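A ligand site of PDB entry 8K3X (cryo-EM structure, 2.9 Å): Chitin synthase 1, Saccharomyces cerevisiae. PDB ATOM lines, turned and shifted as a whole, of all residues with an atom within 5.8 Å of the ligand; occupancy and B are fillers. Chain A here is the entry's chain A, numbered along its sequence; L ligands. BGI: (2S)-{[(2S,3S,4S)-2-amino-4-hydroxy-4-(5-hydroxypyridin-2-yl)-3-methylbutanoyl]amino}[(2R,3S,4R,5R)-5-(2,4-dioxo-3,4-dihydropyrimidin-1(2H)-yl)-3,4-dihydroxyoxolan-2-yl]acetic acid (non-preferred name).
C of Met 454 touches O30 of the ligand (3.5 Å).
Lys 577 touches the ligand (C to N27, 3.8 Å).
Lys 578 touches the ligand.
Ala 603 touches the ligand (N to O31, 3.7 Å).
Pro 675 touches the ligand.
Ala 677 touches the ligand (CB to O11, 3.6 Å).
O of Asp 745 touches N35 of the ligand (3.9 Å).
Trp 760 touches the ligand (CH2 to C06, 3.8 Å).
14 residues have an atom within 4 Å of the ligand: Thr 453, Met 454, Tyr 455, Glu 457, Lys 577, Lys 578, Asp 602, Ala 603, Pro 675, Ala 677, Thr 744, Asp 745, Arg 759 and Trp 760.
The nearest printed residue that does not touch the ligand is Ile 631 (4.1 Å).
An oxygen (O30) of the ligand lies within hydrogen-bond range of the backbone NH (N) of Tyr 455 (3.0 Å).
An oxygen (O31) of the ligand lies within hydrogen-bond range of the backbone carbonyl oxygen (O) of Thr 453, 3.1 Å away.
N15 of the ligand sits close to OD2 of Asp 602 (3.3 Å).
O30 of the ligand sits at hydrogen-bond distance from OE1 of Glu 457, at 2.5 Å.
NH2 of Arg 759 is in salt-bridge range of O33 of the ligand (3.6 Å).
OG1 of Thr 453 lies within hydrogen-bond range of O31 of the ligand (3.4 Å).
The side-chain hydroxyl (OG1) of Thr 744 lies within hydrogen-bond range of an oxygen (O11) of the ligand, 2.6 Å away.
OG1 of Thr 605 is in hydrogen-bond range of OD1 of Asp 602.
The backbone NH of Ala 603 sits at hydrogen-bond distance from the backbone carbonyl oxygen of Thr 453 (2.9 Å).
The side-chain carboxylate (OE2) of Glu 457 sits at hydrogen-bond distance from the backbone NH (N) of Tyr 455, at 2.9 Å.
The side-chain hydroxyl (OG1) of Thr 605 sits at hydrogen-bond distance from the side-chain hydroxyl (OG1) of Thr 744, at 3.5 Å.
OD1 of Asp 745 is in hydrogen-bond range of OG1 of Thr 744 (3.4 Å).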
ATOM      1  N   THR A 453       7.990 -22.911  24.270  1.00  0.00           N
ATOM      2  CA  THR A 453       7.254 -24.162  24.494  1.00  0.00           C
ATOM      3  C   THR A 453       7.837 -24.948  25.668  1.00  0.00           C
ATOM      4  O   THR A 453       9.061 -25.064  25.703  1.00  0.00           O
ATOM      5  CB  THR A 453       7.321 -25.036  23.244  1.00  0.00           C
ATOM      6  OG1 THR A 453       8.703 -25.260  22.971  1.00  0.00           O
ATOM      7  CG2 THR A 453       6.650 -24.408  22.048  1.00  0.00           C
ATOM      8  N   MET A 454       6.994 -25.494  26.544  1.00  0.00           N
ATOM      9  CA  MET A 454       7.456 -26.339  27.673  1.00  0.00           C
ATOM     10  C   MET A 454       6.435 -27.448  27.943  1.00  0.00           C
ATOM     11  O   MET A 454       5.248 -27.203  27.722  1.00  0.00           O
ATOM     12  CB  MET A 454       7.640 -25.510  28.941  1.00  0.00           C
ATOM     13  CG  MET A 454       6.422 -24.739  29.366  1.00  0.00           C
ATOM     14  SD  MET A 454       6.719 -23.995  30.986  1.00  0.00           S
ATOM     15  CE  MET A 454       6.987 -25.473  31.966  1.00  0.00           C
ATOM     16  N   TYR A 455       6.882 -28.612  28.400  1.00  0.00           N
ATOM     17  CA  TYR A 455       6.017 -29.748  28.713  1.00  0.00           C
ATOM     18  C   TYR A 455       6.153 -30.190  30.153  1.00  0.00           C
ATOM     19  O   TYR A 455       5.203 -30.053  30.927  1.00  0.00           O
ATOM     20  CB  TYR A 455       6.330 -30.892  27.762  1.00  0.00           C
ATOM     21  CG  TYR A 455       5.667 -32.195  28.118  1.00  0.00           C
ATOM     22  CD1 TYR A 455       6.409 -33.337  28.336  1.00  0.00           C
ATOM     23  CD2 TYR A 455       4.288 -32.290  28.191  1.00  0.00           C
ATOM     24  CE1 TYR A 455       5.811 -34.526  28.643  1.00  0.00           C
ATOM     25  CE2 TYR A 455       3.685 -33.477  28.489  1.00  0.00           C
ATOM     26  CZ  TYR A 455       4.447 -34.595  28.716  1.00  0.00           C
ATOM     27  OH  TYR A 455       3.851 -35.797  29.017  1.00  0.00           O
ATOM     28  N   ASN A 456       7.326 -30.690  30.553  1.00  0.00           N
ATOM     29  CA  ASN A 456       7.569 -31.098  31.930  1.00  0.00           C
ATOM     30  C   ASN A 456       8.985 -30.786  32.363  1.00  0.00           C
ATOM     31  O   ASN A 456       9.508 -31.447  33.263  1.00  0.00           O
ATOM     32  CB  ASN A 456       7.315 -32.587  32.129  1.00  0.00           C
ATOM     33  CG  ASN A 456       8.078 -33.441  31.150  1.00  0.00           C
ATOM     34  OD1 ASN A 456       8.894 -32.948  30.382  1.00  0.00           O
ATOM     35  ND2 ASN A 456       7.811 -34.740  31.178  1.00  0.00           N
ATOM     36  N   GLU A 457       9.643 -29.832  31.728  1.00  0.00           N
ATOM     37  CA  GLU A 457      11.004 -29.467  32.103  1.00  0.00           C
ATOM     38  C   GLU A 457      10.999 -28.934  33.531  1.00  0.00           C
ATOM     39  O   GLU A 457      10.050 -28.285  33.963  1.00  0.00           O
ATOM     40  CB  GLU A 457      11.561 -28.424  31.147  1.00  0.00           C
ATOM     41  CG  GLU A 457      11.851 -28.941  29.760  1.00  0.00           C
ATOM     42  CD  GLU A 457      10.620 -29.011  28.897  1.00  0.00           C
ATOM     43  OE1 GLU A 457      10.576 -29.848  27.978  1.00  0.00           O
ATOM     44  OE2 GLU A 457       9.677 -28.239  29.160  1.00  0.00           O
ATOM     45  N   ASP A 500       1.859 -26.884  28.813  1.00  0.00           N
ATOM     46  CA  ASP A 500       1.070 -27.876  28.103  1.00  0.00           C
ATOM     47  C   ASP A 500       0.554 -28.896  29.115  1.00  0.00           C
ATOM     48  O   ASP A 500       1.212 -29.890  29.406  1.00  0.00           O
ATOM     49  CB  ASP A 500       1.918 -28.514  27.011  1.00  0.00           C
ATOM     50  N   ASN A 575      -2.353 -32.207  27.377  1.00  0.00           N
ATOM     51  CA  ASN A 575      -1.248 -32.313  26.390  1.00  0.00           C
ATOM     52  C   ASN A 575      -1.844 -32.532  24.995  1.00  0.00           C
ATOM     53  O   ASN A 575      -2.520 -33.553  24.812  1.00  0.00           O
ATOM     54  CB  ASN A 575      -0.268 -33.447  26.699  1.00  0.00           C
ATOM     55  N   LYS A 577       0.311 -32.076  22.243  1.00  0.00           N
ATOM     56  CA  LYS A 577       1.541 -32.204  21.416  1.00  0.00           C
ATOM     57  C   LYS A 577       2.054 -30.798  21.060  1.00  0.00           C
ATOM     58  O   LYS A 577       1.310 -29.850  21.299  1.00  0.00           O
ATOM     59  CB  LYS A 577       1.249 -33.100  20.215  1.00  0.00           C
ATOM     60  N   LYS A 578       3.279 -30.675  20.534  1.00  0.00           N
ATOM     61  CA  LYS A 578       3.844 -29.320  20.264  1.00  0.00           C
ATOM     62  C   LYS A 578       3.046 -28.611  19.168  1.00  0.00           C
ATOM     63  O   LYS A 578       2.832 -27.405  19.309  1.00  0.00           O
ATOM     64  CB  LYS A 578       5.316 -29.399  19.863  1.00  0.00           C
ATOM     65  N   SER A 581       0.505 -26.331  20.523  1.00  0.00           N
ATOM     66  CA  SER A 581       1.074 -25.163  21.214  1.00  0.00           C
ATOM     67  C   SER A 581       1.403 -24.109  20.167  1.00  0.00           C
ATOM     68  O   SER A 581       1.011 -22.954  20.361  1.00  0.00           O
ATOM     69  CB  SER A 581       2.279 -25.567  22.000  1.00  0.00           C
ATOM     70  N   ASP A 602      12.680 -22.899  23.000  1.00  0.00           N
ATOM     71  CA  ASP A 602      12.127 -24.159  23.559  1.00  0.00           C
ATOM     72  C   ASP A 602      12.766 -24.384  24.929  1.00  0.00           C
ATOM     73  O   ASP A 602      14.000 -24.313  25.043  1.00  0.00           O
ATOM     74  CB  ASP A 602      12.280 -25.354  22.613  1.00  0.00           C
ATOM     75  CG  ASP A 602      13.715 -25.754  22.372  1.00  0.00           C
ATOM     76  OD1 ASP A 602      14.609 -24.920  22.595  1.00  0.00           O
ATOM     77  OD2 ASP A 602      13.937 -26.908  21.953  1.00  0.00           O
ATOM     78  N   ALA A 603      11.921 -24.612  25.920  1.00  0.00           N
ATOM     79  CA  ALA A 603      12.371 -24.575  27.306  1.00  0.00           C
ATOM     80  C   ALA A 603      13.586 -25.472  27.505  1.00  0.00           C
ATOM     81  O   ALA A 603      13.568 -26.656  27.170  1.00  0.00           O
ATOM     82  CB  ALA A 603      11.245 -25.014  28.239  1.00  0.00           C
ATOM     83  N   THR A 605      16.594 -24.186  26.252  1.00  0.00           N
ATOM     84  CA  THR A 605      17.519 -23.570  25.326  1.00  0.00           C
ATOM     85  C   THR A 605      17.824 -22.155  25.784  1.00  0.00           C
ATOM     86  O   THR A 605      16.904 -21.374  26.036  1.00  0.00           O
ATOM     87  CB  THR A 605      16.936 -23.557  23.927  1.00  0.00           C
ATOM     88  OG1 THR A 605      16.864 -24.892  23.431  1.00  0.00           O
ATOM     89  CG2 THR A 605      17.782 -22.738  23.005  1.00  0.00           C
ATOM     90  N   ILE A 631      23.075 -23.880  17.102  1.00  0.00           N
ATOM     91  CA  ILE A 631      22.727 -24.616  18.312  1.00  0.00           C
ATOM     92  C   ILE A 631      23.979 -25.307  18.808  1.00  0.00           C
ATOM     93  O   ILE A 631      24.587 -26.100  18.085  1.00  0.00           O
ATOM     94  CB  ILE A 631      21.606 -25.635  18.066  1.00  0.00           C
ATOM     95  CG1 ILE A 631      20.351 -24.954  17.556  1.00  0.00           C
ATOM     96  CG2 ILE A 631      21.267 -26.319  19.323  1.00  0.00           C
ATOM     97  CD1 ILE A 631      19.795 -23.985  18.510  1.00  0.00           C
ATOM     98  N   TYR A 654      26.706 -31.686  15.804  1.00  0.00           N
ATOM     99  CA  TYR A 654      26.064 -30.383  15.711  1.00  0.00           C
ATOM    100  C   TYR A 654      27.008 -29.368  15.120  1.00  0.00           C
ATOM    101  O   TYR A 654      26.607 -28.523  14.303  1.00  0.00           O
ATOM    102  CB  TYR A 654      25.619 -29.896  17.096  1.00  0.00           C
ATOM    103  CG  TYR A 654      24.419 -30.601  17.672  1.00  0.00           C
ATOM    104  CD1 TYR A 654      23.781 -31.607  16.990  1.00  0.00           C
ATOM    105  CD2 TYR A 654      23.926 -30.236  18.901  1.00  0.00           C
ATOM    106  CE1 TYR A 654      22.697 -32.238  17.522  1.00  0.00           C
ATOM    107  CE2 TYR A 654      22.840 -30.866  19.447  1.00  0.00           C
ATOM    108  CZ  TYR A 654      22.232 -31.866  18.748  1.00  0.00           C
ATOM    109  OH  TYR A 654      21.139 -32.481  19.292  1.00  0.00           O
ATOM    110  N   PRO A 675      15.841 -25.080  13.176  1.00  0.00           N
ATOM    111  CA  PRO A 675      15.590 -25.846  14.391  1.00  0.00           C
ATOM    112  C   PRO A 675      14.520 -25.190  15.234  1.00  0.00           C
ATOM    113  O   PRO A 675      14.491 -23.970  15.391  1.00  0.00           O
ATOM    114  CB  PRO A 675      16.942 -25.830  15.092  1.00  0.00           C
ATOM    115  CG  PRO A 675      17.591 -24.622  14.605  1.00  0.00           C
ATOM    116  CD  PRO A 675      17.196 -24.517  13.172  1.00  0.00           C
ATOM    117  N   GLY A 676      13.639 -26.000  15.781  1.00  0.00           N
ATOM    118  CA  GLY A 676      12.588 -25.456  16.601  1.00  0.00           C
ATOM    119  C   GLY A 676      13.015 -24.975  17.950  1.00  0.00           C
ATOM    120  O   GLY A 676      12.242 -24.354  18.668  1.00  0.00           O
ATOM    121  N   ALA A 677      14.268 -25.245  18.329  1.00  0.00           N
ATOM    122  CA  ALA A 677      14.795 -24.795  19.597  1.00  0.00           C
ATOM    123  C   ALA A 677      15.214 -23.339  19.567  1.00  0.00           C
ATOM    124  O   ALA A 677      15.261 -22.697  20.626  1.00  0.00           O
ATOM    125  CB  ALA A 677      15.996 -25.651  19.999  1.00  0.00           C
ATOM    126  N   THR A 744      21.794 -25.788  23.992  1.00  0.00           N
ATOM    127  CA  THR A 744      20.720 -26.686  24.385  1.00  0.00           C
ATOM    128  C   THR A 744      21.280 -27.924  25.077  1.00  0.00           C
ATOM    129  O   THR A 744      22.481 -28.176  25.070  1.00  0.00           O
ATOM    130  CB  THR A 744      19.889 -27.097  23.176  1.00  0.00           C
ATOM    131  OG1 THR A 744      18.728 -27.801  23.622  1.00  0.00           O
ATOM    132  CG2 THR A 744      20.690 -28.017  22.310  1.00  0.00           C
ATOM    133  N   ASP A 745      20.392 -28.696  25.678  1.00  0.00           N
ATOM    134  CA  ASP A 745      20.746 -29.947  26.343  1.00  0.00           C
ATOM    135  C   ASP A 745      20.474 -31.116  25.415  1.00  0.00           C
ATOM    136  O   ASP A 745      19.483 -31.112  24.688  1.00  0.00           O
ATOM    137  CB  ASP A 745      19.953 -30.124  27.633  1.00  0.00           C
ATOM    138  CG  ASP A 745      18.462 -30.067  27.399  1.00  0.00           C
ATOM    139  OD1 ASP A 745      18.005 -29.146  26.688  1.00  0.00           O
ATOM    140  OD2 ASP A 745      17.740 -30.928  27.921  1.00  0.00           O
ATOM    141  N   GLN A 756      14.893 -39.962  20.228  1.00  0.00           N
ATOM    142  CA  GLN A 756      14.936 -38.608  19.688  1.00  0.00           C
ATOM    143  C   GLN A 756      15.233 -38.628  18.192  1.00  0.00           C
ATOM    144  O   GLN A 756      14.567 -37.935  17.423  1.00  0.00           O
ATOM    145  CB  GLN A 756      15.979 -37.776  20.413  1.00  0.00           C
ATOM    146  CG  GLN A 756      16.219 -36.460  19.744  1.00  0.00           C
ATOM    147  CD  GLN A 756      17.403 -35.738  20.302  1.00  0.00           C
ATOM    148  OE1 GLN A 756      18.541 -36.046  19.965  1.00  0.00           O
ATOM    149  NE2 GLN A 756      17.153 -34.786  21.166  1.00  0.00           N
ATOM    150  N   ARG A 759      12.574 -39.386  15.407  1.00  0.00           N
ATOM    151  CA  ARG A 759      11.764 -38.309  14.859  1.00  0.00           C
ATOM    152  C   ARG A 759      12.500 -37.567  13.760  1.00  0.00           C
ATOM    153  O   ARG A 759      11.932 -37.279  12.705  1.00  0.00           O
ATOM    154  CB  ARG A 759      11.361 -37.344  15.963  1.00  0.00           C
ATOM    155  CG  ARG A 759      10.298 -37.852  16.884  1.00  0.00           C
ATOM    156  CD  ARG A 759       9.568 -36.708  17.539  1.00  0.00           C
ATOM    157  NE  ARG A 759      10.442 -35.567  17.753  1.00  0.00           N
ATOM    158  CZ  ARG A 759      11.138 -35.367  18.864  1.00  0.00           C
ATOM    159  NH1 ARG A 759      11.048 -36.231  19.857  1.00  0.00           N
ATOM    160  NH2 ARG A 759      11.918 -34.300  18.989  1.00  0.00           N
ATOM    161  N   TRP A 760      13.771 -37.244  13.994  1.00  0.00           N
ATOM    162  CA  TRP A 760      14.522 -36.442  13.050  1.00  0.00           C
ATOM    163  C   TRP A 760      14.711 -37.166  11.729  1.00  0.00           C
ATOM    164  O   TRP A 760      14.569 -36.563  10.669  1.00  0.00           O
ATOM    165  CB  TRP A 760      15.880 -36.076  13.619  1.00  0.00           C
ATOM    166  CG  TRP A 760      15.847 -35.198  14.802  1.00  0.00           C
ATOM    167  CD1 TRP A 760      14.776 -34.893  15.569  1.00  0.00           C
ATOM    168  CD2 TRP A 760      16.960 -34.505  15.357  1.00  0.00           C
ATOM    169  NE1 TRP A 760      15.153 -34.054  16.581  1.00  0.00           N
ATOM    170  CE2 TRP A 760      16.489 -33.799  16.465  1.00  0.00           C
ATOM    171  CE3 TRP A 760      18.311 -34.417  15.021  1.00  0.00           C
ATOM    172  CZ2 TRP A 760      17.320 -33.023  17.237  1.00  0.00           C
ATOM    173  CZ3 TRP A 760      19.120 -33.640  15.783  1.00  0.00           C
ATOM    174  CH2 TRP A 760      18.630 -32.958  16.882  1.00  0.00           C
HETATM  175  C13 BGI L   1      13.498 -30.175  22.858  1.00  0.00           C
HETATM  176  C17 BGI L   1      10.132 -29.331  22.767  1.00  0.00           C
HETATM  177  C20 BGI L   1       8.097 -29.597  23.786  1.00  0.00           C
HETATM  178  C24 BGI L   1       6.360 -32.946  24.466  1.00  0.00           C
HETATM  179  C28 BGI L   1       5.609 -30.160  23.651  1.00  0.00           C
HETATM  180  C01 BGI L   1      14.672 -30.963  20.561  1.00  0.00           C
HETATM  181  C02 BGI L   1      15.230 -29.675  21.117  1.00  0.00           C
HETATM  182  C03 BGI L   1      16.745 -29.653  20.917  1.00  0.00           C
HETATM  183  C04 BGI L   1      17.116 -29.474  19.430  1.00  0.00           C
HETATM  184  C06 BGI L   1      18.789 -29.271  17.858  1.00  0.00           C
HETATM  185  C07 BGI L   1      17.859 -29.186  16.831  1.00  0.00           C
HETATM  186  C08 BGI L   1      16.511 -29.242  17.114  1.00  0.00           C
HETATM  187  C09 BGI L   1      16.133 -29.393  18.446  1.00  0.00           C
HETATM  188  C12 BGI L   1      14.895 -29.589  22.608  1.00  0.00           C
HETATM  189  C16 BGI L   1      10.988 -30.350  22.295  1.00  0.00           C
HETATM  190  C18 BGI L   1      10.410 -29.122  24.310  1.00  0.00           C
HETATM  191  C19 BGI L   1       9.264 -29.845  24.933  1.00  0.00           C
HETATM  192  C23 BGI L   1       7.392 -31.935  24.316  1.00  0.00           C
HETATM  193  C25 BGI L   1       4.976 -32.605  24.224  1.00  0.00           C
HETATM  194  C32 BGI L   1      10.443 -30.949  20.965  1.00  0.00           C
HETATM  195  N05 BGI L   1      18.390 -29.412  19.120  1.00  0.00           N
HETATM  196  N15 BGI L   1      12.359 -29.761  22.025  1.00  0.00           N
HETATM  197  N22 BGI L   1       7.038 -30.570  23.929  1.00  0.00           N
HETATM  198  N27 BGI L   1       4.590 -31.269  23.834  1.00  0.00           N
HETATM  199  N35 BGI L   1      15.875 -30.349  23.351  1.00  0.00           N
HETATM  200  O10 BGI L   1      18.305 -29.025  15.511  1.00  0.00           O
HETATM  201  O11 BGI L   1      17.277 -28.601  21.641  1.00  0.00           O
HETATM  202  O14 BGI L   1      13.335 -30.965  23.724  1.00  0.00           O
HETATM  203  O21 BGI L   1       8.676 -29.748  22.661  1.00  0.00           O
HETATM  204  O26 BGI L   1       4.143 -33.440  24.350  1.00  0.00           O
HETATM  205  O29 BGI L   1       5.309 -29.075  23.334  1.00  0.00           O
HETATM  206  O30 BGI L   1       8.899 -29.220  26.218  1.00  0.00           O
HETATM  207  O31 BGI L   1      10.347 -27.656  24.663  1.00  0.00           O
HETATM  208  O33 BGI L   1      11.128 -30.885  19.918  1.00  0.00           O
HETATM  209  O34 BGI L   1       9.323 -31.526  20.946  1.00  0.00           O
